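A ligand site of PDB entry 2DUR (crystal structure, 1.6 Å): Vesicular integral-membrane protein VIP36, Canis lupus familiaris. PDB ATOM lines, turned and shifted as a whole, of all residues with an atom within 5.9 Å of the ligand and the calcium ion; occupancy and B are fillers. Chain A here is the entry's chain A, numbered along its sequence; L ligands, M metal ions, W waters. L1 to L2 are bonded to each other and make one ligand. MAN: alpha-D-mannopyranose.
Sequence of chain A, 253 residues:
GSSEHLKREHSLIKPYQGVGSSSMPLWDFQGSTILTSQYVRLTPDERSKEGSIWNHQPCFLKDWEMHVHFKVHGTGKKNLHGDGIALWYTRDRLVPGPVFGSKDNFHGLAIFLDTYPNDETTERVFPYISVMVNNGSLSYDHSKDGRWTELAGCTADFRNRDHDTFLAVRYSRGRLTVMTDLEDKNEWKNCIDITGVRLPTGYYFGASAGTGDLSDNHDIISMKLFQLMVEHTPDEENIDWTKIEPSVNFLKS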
ATOM      1  N   ARG A  47      23.175  -8.017   2.123  1.00  0.00           N
ATOM      2  CA  ARG A  47      23.450  -8.783   0.914  1.00  0.00           C
ATOM      3  C   ARG A  47      24.653  -9.695   1.071  1.00  0.00           C
ATOM      4  O   ARG A  47      25.549  -9.445   1.887  1.00  0.00           O
ATOM      5  CB  ARG A  47      23.623  -7.805  -0.263  1.00  0.00           C
ATOM      6  CG  ARG A  47      22.326  -7.122  -0.616  1.00  0.00           C
ATOM      7  CD  ARG A  47      22.446  -6.157  -1.764  1.00  0.00           C
ATOM      8  NE  ARG A  47      23.427  -5.126  -1.447  1.00  0.00           N
ATOM      9  CZ  ARG A  47      23.789  -4.173  -2.294  1.00  0.00           C
ATOM     10  NH1 ARG A  47      23.225  -4.107  -3.488  1.00  0.00           N
ATOM     11  NH2 ARG A  47      24.695  -3.293  -1.938  1.00  0.00           N
ATOM     12  N   SER A  48      24.656 -10.763   0.271  1.00  0.00           N
ATOM     13  CA  SER A  48      25.798 -11.675   0.155  1.00  0.00           C
ATOM     14  C   SER A  48      26.268 -12.241   1.487  1.00  0.00           C
ATOM     15  O   SER A  48      27.455 -12.159   1.841  1.00  0.00           O
ATOM     16  CB  SER A  48      26.960 -10.993  -0.608  1.00  0.00           C
ATOM     17  OG  SER A  48      26.513 -10.669  -1.920  1.00  0.00           O
ATOM     18  N   LYS A  49      25.325 -12.853   2.216  1.00  0.00           N
ATOM     19  CA  LYS A  49      25.616 -13.518   3.487  1.00  0.00           C
ATOM     20  C   LYS A  49      25.251 -15.000   3.405  1.00  0.00           C
ATOM     21  O   LYS A  49      24.325 -15.378   2.688  1.00  0.00           O
ATOM     22  CB  LYS A  49      24.819 -12.896   4.648  1.00  0.00           C
ATOM     23  CG  LYS A  49      25.019 -11.377   4.821  1.00  0.00           C
ATOM     24  CD  LYS A  49      26.355 -11.066   5.464  1.00  0.00           C
ATOM     25  CE  LYS A  49      26.569  -9.551   5.521  1.00  0.00           C
ATOM     26  NZ  LYS A  49      27.989  -9.222   5.817  1.00  0.00           N
ATOM     27  N   GLU A  50      26.019 -15.813   4.126  1.00  0.00           N
ATOM     28  CA  GLU A  50      25.712 -17.236   4.269  1.00  0.00           C
ATOM     29  C   GLU A  50      26.047 -17.668   5.667  1.00  0.00           C
ATOM     30  O   GLU A  50      27.183 -17.472   6.138  1.00  0.00           O
ATOM     31  CB  GLU A  50      26.496 -18.055   3.239  1.00  0.00           C
ATOM     32  CG  GLU A  50      25.921 -17.849   1.837  1.00  0.00           C
ATOM     33  CD  GLU A  50      26.739 -18.406   0.694  1.00  0.00           C
ATOM     34  OE1 GLU A  50      27.888 -18.866   0.893  1.00  0.00           O
ATOM     35  OE2 GLU A  50      26.223 -18.353  -0.433  1.00  0.00           O
ATOM     36  N   HIS A  81      13.385  -9.511  -1.977  1.00  0.00           N
ATOM     37  CA  HIS A  81      13.911 -10.143  -0.781  1.00  0.00           C
ATOM     38  C   HIS A  81      14.329 -11.557  -1.146  1.00  0.00           C
ATOM     39  O   HIS A  81      13.938 -12.076  -2.163  1.00  0.00           O
ATOM     40  CB  HIS A  81      12.854 -10.210   0.338  1.00  0.00           C
ATOM     41  CG  HIS A  81      11.613 -10.967  -0.071  1.00  0.00           C
ATOM     42  ND1 HIS A  81      10.462 -10.323  -0.489  1.00  0.00           N
ATOM     43  CD2 HIS A  81      11.379 -12.291  -0.202  1.00  0.00           C
ATOM     44  CE1 HIS A  81       9.565 -11.233  -0.828  1.00  0.00           C
ATOM     45  NE2 HIS A  81      10.095 -12.431  -0.663  1.00  0.00           N
ATOM     46  N   GLY A  82      15.112 -12.166  -0.281  1.00  0.00           N
ATOM     47  CA  GLY A  82      15.597 -13.547  -0.492  1.00  0.00           C
ATOM     48  C   GLY A  82      16.739 -13.884   0.464  1.00  0.00           C
ATOM     49  O   GLY A  82      17.150 -13.044   1.290  1.00  0.00           O
ATOM     50  N   ASP A  83      17.287 -15.105   0.384  1.00  0.00           N
ATOM     51  CA  ASP A  83      16.835 -16.140  -0.551  1.00  0.00           C
ATOM     52  C   ASP A  83      16.049 -17.265   0.115  1.00  0.00           C
ATOM     53  O   ASP A  83      15.294 -17.978  -0.572  1.00  0.00           O
ATOM     54  CB  ASP A  83      18.073 -16.732  -1.249  1.00  0.00           C
ATOM     55  CG  ASP A  83      18.511 -15.862  -2.423  1.00  0.00           C
ATOM     56  OD1 ASP A  83      19.483 -15.065  -2.270  1.00  0.00           O
ATOM     57  OD2 ASP A  83      17.849 -15.947  -3.471  1.00  0.00           O
ATOM     58  N   PHE A 100      21.342 -22.279  -0.123  1.00  0.00           N
ATOM     59  CA  PHE A 100      20.963 -21.510   1.078  1.00  0.00           C
ATOM     60  C   PHE A 100      22.062 -21.512   2.128  1.00  0.00           C
ATOM     61  O   PHE A 100      21.799 -21.661   3.325  1.00  0.00           O
ATOM     62  CB  PHE A 100      19.642 -22.060   1.636  1.00  0.00           C
ATOM     63  CG  PHE A 100      18.552 -22.082   0.621  1.00  0.00           C
ATOM     64  CD1 PHE A 100      17.840 -20.916   0.314  1.00  0.00           C
ATOM     65  CD2 PHE A 100      18.276 -23.245  -0.105  1.00  0.00           C
ATOM     66  CE1 PHE A 100      16.836 -20.913  -0.655  1.00  0.00           C
ATOM     67  CE2 PHE A 100      17.280 -23.244  -1.080  1.00  0.00           C
ATOM     68  CZ  PHE A 100      16.552 -22.097  -1.373  1.00  0.00           C
ATOM     69  N   ASP A 114      12.127 -21.486   0.337  1.00  0.00           N
ATOM     70  CA  ASP A 114      12.668 -20.598  -0.714  1.00  0.00           C
ATOM     71  C   ASP A 114      11.723 -19.411  -0.866  1.00  0.00           C
ATOM     72  O   ASP A 114      10.551 -19.600  -1.167  1.00  0.00           O
ATOM     73  CB  ASP A 114      12.762 -21.418  -2.025  1.00  0.00           C
ATOM     74  CG  ASP A 114      13.449 -20.661  -3.162  1.00  0.00           C
ATOM     75  OD1 ASP A 114      13.804 -21.307  -4.195  1.00  0.00           O
ATOM     76  OD2 ASP A 114      13.626 -19.434  -3.043  1.00  0.00           O
ATOM     77  N   THR A 115      12.223 -18.188  -0.679  1.00  0.00           N
ATOM     78  CA  THR A 115      11.381 -16.998  -0.690  1.00  0.00           C
ATOM     79  C   THR A 115      11.470 -16.162  -1.961  1.00  0.00           C
ATOM     80  O   THR A 115      10.773 -15.167  -2.102  1.00  0.00           O
ATOM     81  CB  THR A 115      11.744 -16.063   0.463  1.00  0.00           C
ATOM     82  OG1 THR A 115      13.112 -15.667   0.318  1.00  0.00           O
ATOM     83  CG2 THR A 115      11.571 -16.730   1.849  1.00  0.00           C
ATOM     84  N   TYR A 116      12.341 -16.543  -2.906  1.00  0.00           N
ATOM     85  CA  TYR A 116      12.546 -15.734  -4.099  1.00  0.00           C
ATOM     86  C   TYR A 116      12.479 -16.590  -5.371  1.00  0.00           C
ATOM     87  O   TYR A 116      13.275 -17.518  -5.497  1.00  0.00           O
ATOM     88  CB  TYR A 116      13.912 -15.037  -4.039  1.00  0.00           C
ATOM     89  CG  TYR A 116      14.190 -14.231  -5.268  1.00  0.00           C
ATOM     90  CD1 TYR A 116      13.402 -13.118  -5.602  1.00  0.00           C
ATOM     91  CD2 TYR A 116      15.243 -14.576  -6.122  1.00  0.00           C
ATOM     92  CE1 TYR A 116      13.655 -12.392  -6.751  1.00  0.00           C
ATOM     93  CE2 TYR A 116      15.501 -13.838  -7.281  1.00  0.00           C
ATOM     94  CZ  TYR A 116      14.683 -12.757  -7.585  1.00  0.00           C
ATOM     95  OH  TYR A 116      14.930 -12.020  -8.725  1.00  0.00           O
ATOM     96  N   PRO A 117      11.549 -16.290  -6.319  1.00  0.00           N
ATOM     97  CA  PRO A 117      11.518 -17.093  -7.550  1.00  0.00           C
ATOM     98  C   PRO A 117      12.634 -16.697  -8.518  1.00  0.00           C
ATOM     99  O   PRO A 117      12.518 -15.694  -9.227  1.00  0.00           O
ATOM    100  CB  PRO A 117      10.133 -16.790  -8.152  1.00  0.00           C
ATOM    101  CG  PRO A 117       9.728 -15.466  -7.567  1.00  0.00           C
ATOM    102  CD  PRO A 117      10.485 -15.259  -6.287  1.00  0.00           C
ATOM    103  N   ASN A 118      13.710 -17.484  -8.539  1.00  0.00           N
ATOM    104  CA  ASN A 118      14.802 -17.251  -9.481  1.00  0.00           C
ATOM    105  C   ASN A 118      14.380 -17.634 -10.904  1.00  0.00           C
ATOM    106  O   ASN A 118      14.906 -17.097 -11.887  1.00  0.00           O
ATOM    107  CB  ASN A 118      16.011 -18.080  -9.090  1.00  0.00           C
ATOM    108  CG  ASN A 118      16.623 -17.621  -7.809  1.00  0.00           C
ATOM    109  OD1 ASN A 118      16.201 -18.024  -6.723  1.00  0.00           O
ATOM    110  ND2 ASN A 118      17.650 -16.790  -7.911  1.00  0.00           N
ATOM    111  N   PHE A 126       5.393 -18.476  -4.723  1.00  0.00           N
ATOM    112  CA  PHE A 126       6.369 -18.342  -3.627  1.00  0.00           C
ATOM    113  C   PHE A 126       5.811 -17.561  -2.416  1.00  0.00           C
ATOM    114  O   PHE A 126       4.833 -16.806  -2.581  1.00  0.00           O
ATOM    115  CB  PHE A 126       7.692 -17.728  -4.141  1.00  0.00           C
ATOM    116  CG  PHE A 126       8.501 -18.692  -4.959  1.00  0.00           C
ATOM    117  CD1 PHE A 126       8.049 -19.129  -6.194  1.00  0.00           C
ATOM    118  CD2 PHE A 126       9.704 -19.202  -4.457  1.00  0.00           C
ATOM    119  CE1 PHE A 126       8.784 -20.065  -6.949  1.00  0.00           C
ATOM    120  CE2 PHE A 126      10.441 -20.144  -5.190  1.00  0.00           C
ATOM    121  CZ  PHE A 126       9.992 -20.578  -6.438  1.00  0.00           C
ATOM    122  N   TYR A 140      21.580 -28.796  -6.691  1.00  0.00           N
ATOM    123  CA  TYR A 140      20.415 -27.935  -6.599  1.00  0.00           C
ATOM    124  C   TYR A 140      20.606 -26.791  -7.575  1.00  0.00           C
ATOM    125  O   TYR A 140      21.567 -26.015  -7.451  1.00  0.00           O
ATOM    126  CB  TYR A 140      20.298 -27.425  -5.168  1.00  0.00           C
ATOM    127  CG  TYR A 140      19.241 -26.376  -4.976  1.00  0.00           C
ATOM    128  CD1 TYR A 140      17.888 -26.745  -4.866  1.00  0.00           C
ATOM    129  CD2 TYR A 140      19.591 -25.024  -4.844  1.00  0.00           C
ATOM    130  CE1 TYR A 140      16.907 -25.792  -4.656  1.00  0.00           C
ATOM    131  CE2 TYR A 140      18.619 -24.050  -4.642  1.00  0.00           C
ATOM    132  CZ  TYR A 140      17.284 -24.439  -4.555  1.00  0.00           C
ATOM    133  OH  TYR A 140      16.287 -23.519  -4.363  1.00  0.00           O
ATOM    134  N   HIS A 142      20.005 -23.536  -8.380  1.00  0.00           N
ATOM    135  CA  HIS A 142      19.481 -22.380  -7.643  1.00  0.00           C
ATOM    136  C   HIS A 142      18.720 -21.435  -8.563  1.00  0.00           C
ATOM    137  O   HIS A 142      17.652 -20.912  -8.235  1.00  0.00           O
ATOM    138  CB  HIS A 142      20.625 -21.655  -6.937  1.00  0.00           C
ATOM    139  CG  HIS A 142      20.202 -20.393  -6.266  1.00  0.00           C
ATOM    140  ND1 HIS A 142      19.644 -20.367  -5.005  1.00  0.00           N
ATOM    141  CD2 HIS A 142      20.180 -19.107  -6.701  1.00  0.00           C
ATOM    142  CE1 HIS A 142      19.336 -19.129  -4.684  1.00  0.00           C
ATOM    143  NE2 HIS A 142      19.643 -18.349  -5.699  1.00  0.00           N
ATOM    144  N   ASP A 145      15.188 -22.540  -8.941  1.00  0.00           N
ATOM    145  CA  ASP A 145      14.557 -22.878  -7.656  1.00  0.00           C
ATOM    146  C   ASP A 145      14.497 -24.411  -7.447  1.00  0.00           C
ATOM    147  O   ASP A 145      13.506 -24.940  -6.917  1.00  0.00           O
ATOM    148  CB  ASP A 145      13.149 -22.269  -7.553  1.00  0.00           C
ATOM    149  CG  ASP A 145      13.147 -20.782  -7.874  1.00  0.00           C
ATOM    150  OD1 ASP A 145      12.461 -20.375  -8.828  1.00  0.00           O
ATOM    151  OD2 ASP A 145      13.888 -20.041  -7.229  1.00  0.00           O
ATOM    152  N   THR A 211      21.685 -15.039   1.551  1.00  0.00           N
ATOM    153  CA  THR A 211      21.201 -13.820   0.883  1.00  0.00           C
ATOM    154  C   THR A 211      22.178 -13.566  -0.271  1.00  0.00           C
ATOM    155  O   THR A 211      23.349 -13.938  -0.174  1.00  0.00           O
ATOM    156  CB  THR A 211      21.199 -12.582   1.846  1.00  0.00           C
ATOM    157  OG1 THR A 211      22.514 -12.357   2.355  1.00  0.00           O
ATOM    158  CG2 THR A 211      20.260 -12.861   3.040  1.00  0.00           C
ATOM    159  N   GLY A 212      21.688 -12.958  -1.347  1.00  0.00           N
ATOM    160  CA  GLY A 212      22.510 -12.643  -2.536  1.00  0.00           C
ATOM    161  C   GLY A 212      22.376 -11.157  -2.782  1.00  0.00           C
ATOM    162  O   GLY A 212      22.724 -10.351  -1.919  1.00  0.00           O
ATOM    163  N   ASP A 213      21.894 -10.802  -3.977  1.00  0.00           N
ATOM    164  CA  ASP A 213      21.603  -9.398  -4.289  1.00  0.00           C
ATOM    165  C   ASP A 213      20.370  -8.951  -3.511  1.00  0.00           C
ATOM    166  O   ASP A 213      20.098  -7.728  -3.445  1.00  0.00           O
ATOM    167  CB  ASP A 213      21.329  -9.231  -5.783  1.00  0.00           C
ATOM    168  CG  ASP A 213      22.561  -9.496  -6.626  1.00  0.00           C
ATOM    169  OD1 ASP A 213      23.677  -9.266  -6.136  1.00  0.00           O
ATOM    170  OD2 ASP A 213      22.384  -9.922  -7.791  1.00  0.00           O
ATOM    171  N   LEU A 214      19.620  -9.926  -2.989  1.00  0.00           N
ATOM    172  CA  LEU A 214      18.419  -9.681  -2.151  1.00  0.00           C
ATOM    173  C   LEU A 214      18.623 -10.307  -0.802  1.00  0.00           C
ATOM    174  O   LEU A 214      19.385 -11.268  -0.662  1.00  0.00           O
ATOM    175  CB  LEU A 214      17.192 -10.274  -2.840  1.00  0.00           C
ATOM    176  CG  LEU A 214      16.887  -9.741  -4.246  1.00  0.00           C
ATOM    177  CD1 LEU A 214      15.718 -10.482  -4.865  1.00  0.00           C
ATOM    178  CD2 LEU A 214      16.638  -8.228  -4.193  1.00  0.00           C
ATOM    179  N   SER A 215      17.938  -9.786   0.206  1.00  0.00           N
ATOM    180  CA  SER A 215      18.233 -10.223   1.550  1.00  0.00           C
ATOM    181  C   SER A 215      16.957 -10.306   2.404  1.00  0.00           C
ATOM    182  O   SER A 215      15.864  -9.962   1.940  1.00  0.00           O
ATOM    183  CB  SER A 215      19.261  -9.293   2.202  1.00  0.00           C
ATOM    184  OG  SER A 215      18.702  -8.001   2.392  1.00  0.00           O
HETATM  185  C1  MAN L   1      21.991 -12.824  -6.989  1.00  0.00           C
HETATM  186  C2  MAN L   1      22.402 -14.289  -7.049  1.00  0.00           C
HETATM  187  C3  MAN L   1      21.172 -15.198  -6.941  1.00  0.00           C
HETATM  188  C4  MAN L   1      20.272 -14.809  -5.764  1.00  0.00           C
HETATM  189  C5  MAN L   1      19.861 -13.363  -5.975  1.00  0.00           C
HETATM  190  C6  MAN L   1      18.885 -12.889  -4.899  1.00  0.00           C
HETATM  191  O1  MAN L   1      21.483 -12.397  -8.248  1.00  0.00           O
HETATM  192  O2  MAN L   1      23.257 -14.552  -5.954  1.00  0.00           O
HETATM  193  O3  MAN L   1      21.584 -16.556  -6.844  1.00  0.00           O
HETATM  194  O4  MAN L   1      19.115 -15.627  -5.673  1.00  0.00           O
HETATM  195  O5  MAN L   1      21.052 -12.608  -5.925  1.00  0.00           O
HETATM  196  O6  MAN L   1      19.547 -12.808  -3.645  1.00  0.00           O
HETATM  197  C1  MAN L   2      24.603 -14.735  -6.414  1.00  0.00           C
HETATM  198  C2  MAN L   2      25.271 -15.707  -5.446  1.00  0.00           C
HETATM  199  C3  MAN L   2      25.375 -15.031  -4.079  1.00  0.00           C
HETATM  200  C4  MAN L   2      26.051 -13.662  -4.184  1.00  0.00           C
HETATM  201  C5  MAN L   2      25.399 -12.793  -5.267  1.00  0.00           C
HETATM  202  C6  MAN L   2      26.175 -11.505  -5.545  1.00  0.00           C
HETATM  203  O2  MAN L   2      26.556 -16.002  -5.973  1.00  0.00           O
HETATM  204  O3  MAN L   2      26.075 -15.888  -3.205  1.00  0.00           O
HETATM  205  O4  MAN L   2      25.977 -13.038  -2.933  1.00  0.00           O
HETATM  206  O5  MAN L   2      25.356 -13.534  -6.472  1.00  0.00           O
HETATM  207  O6  MAN L   2      25.646 -10.822  -6.686  1.00  0.00           O
HETATM  208 CA    CA M   1      14.849 -19.262  -5.212  1.00  0.00          CA
HETATM  209  O   HOH W   1      16.632 -20.922  -5.455  1.00  0.00           O
HETATM  210  O   HOH W   2      19.375 -13.437  -9.888  1.00  0.00           O
HETATM  211  O   HOH W   3      16.096 -18.041  -3.503  1.00  0.00           O
HETATM  212  O   HOH W   4      22.508 -17.272  -4.509  1.00  0.00           O
HETATM  213  O   HOH W   5      27.791 -14.155  -1.189  1.00  0.00           O
HETATM  214  O   HOH W   6      28.747 -16.035  -3.232  1.00  0.00           O
HETATM  215  O   HOH W   7      24.509 -16.388  -0.723  1.00  0.00           O
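N of Asp 213 is in hydrogen-bond range of O5 of MAN L1.
O6 of MAN L1 lies within hydrogen-bond range of O of Leu 214 (3.4 Å).
NE2 of His 142 lies within hydrogen-bond range of O4 of MAN L1 (2.8 Å).
The side-chain carboxylate (OD2) of Asp 83 is in hydrogen-bond range of an oxygen (O4) of MAN L1, at 2.6 Å.
An oxygen (O4) of MAN L2 is in hydrogen-bond range of the side-chain hydroxyl (OG) of Ser 48, 2.6 Å away.
The backbone NH (N) of Leu 214 is in hydrogen-bond range of an oxygen (O6) of MAN L1.
ND2 of Asn 118 is in hydrogen-bond range of O4 of MAN L1, at 2.9 Å.
The backbone NH of Gly 212 sits at hydrogen-bond distance from an oxygen (O6) of MAN L1 (3.1 Å).
The side-chain carboxylate of Asp 213 sits at hydrogen-bond distance from an oxygen (O6) of MAN L2, at 2.6 Å.
The side-chain hydroxyl (OG1) of Thr 211 lies within hydrogen-bond range of the backbone NH (N) of Ser 48 (3.4 Å).
N of Lys 49 lies within hydrogen-bond range of OG1 of Thr 211.
The backbone NH (N) of Gly 212 is in hydrogen-bond range of the side-chain carboxylate (OD1) of Asp 83, at 3.2 Å.
N of Ser 48 lies within hydrogen-bond range of O of Gly 212, at 2.9 Å.
A ring nitrogen (NE2) of His 142 is in hydrogen-bond range of the side-chain amide nitrogen (ND2) of Asn 118, 3.4 Å away.
The backbone carbonyl oxygen of Asp 83 lies within hydrogen-bond range of the backbone NH of Thr 115 (3.1 Å).
OD1 of Asp 114 lies close to OH of Tyr 140, 3.3 Å away.
Residues that only touch the ligand: Glu 50 (3.7 Å) and Thr 211 (3.9 Å).
The nearest printed residue that does not touch the ligand is Tyr 116 (4.04 Å).
Within 4 Å of the calcium ion: Asp 114, Tyr 116, Asn 118 and Asp 145.
The nearest printed residue that does not touch the calcium ion is His 142 (4.4 Å).
The calcium ion is bound by OD2 of Asp 145 (2.4 Å), O of Tyr 116 (2.4 Å), OD1 of Asn 118 (2.4 Å), water W3 (2.4 Å), water W1 (2.4 Å), OD2 of Asp 114 (2.5 Å) and OD1 of Asp 114 (2.5 Å).
Water W1 bridges the side-chain hydroxyl (OH) of Tyr 140 (2.8 Å) and the backbone carbonyl oxygen (O) of His 142 (3.0 Å).
Water W4 bridges O3 of MAN L1 and NE2 of His 142.
Water W7 lies within hydrogen-bond range of OE2 of Glu 50 (2.6 Å), O of Thr 211 (2.8 Å) and O3 of MAN L2 (3.0 Å).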
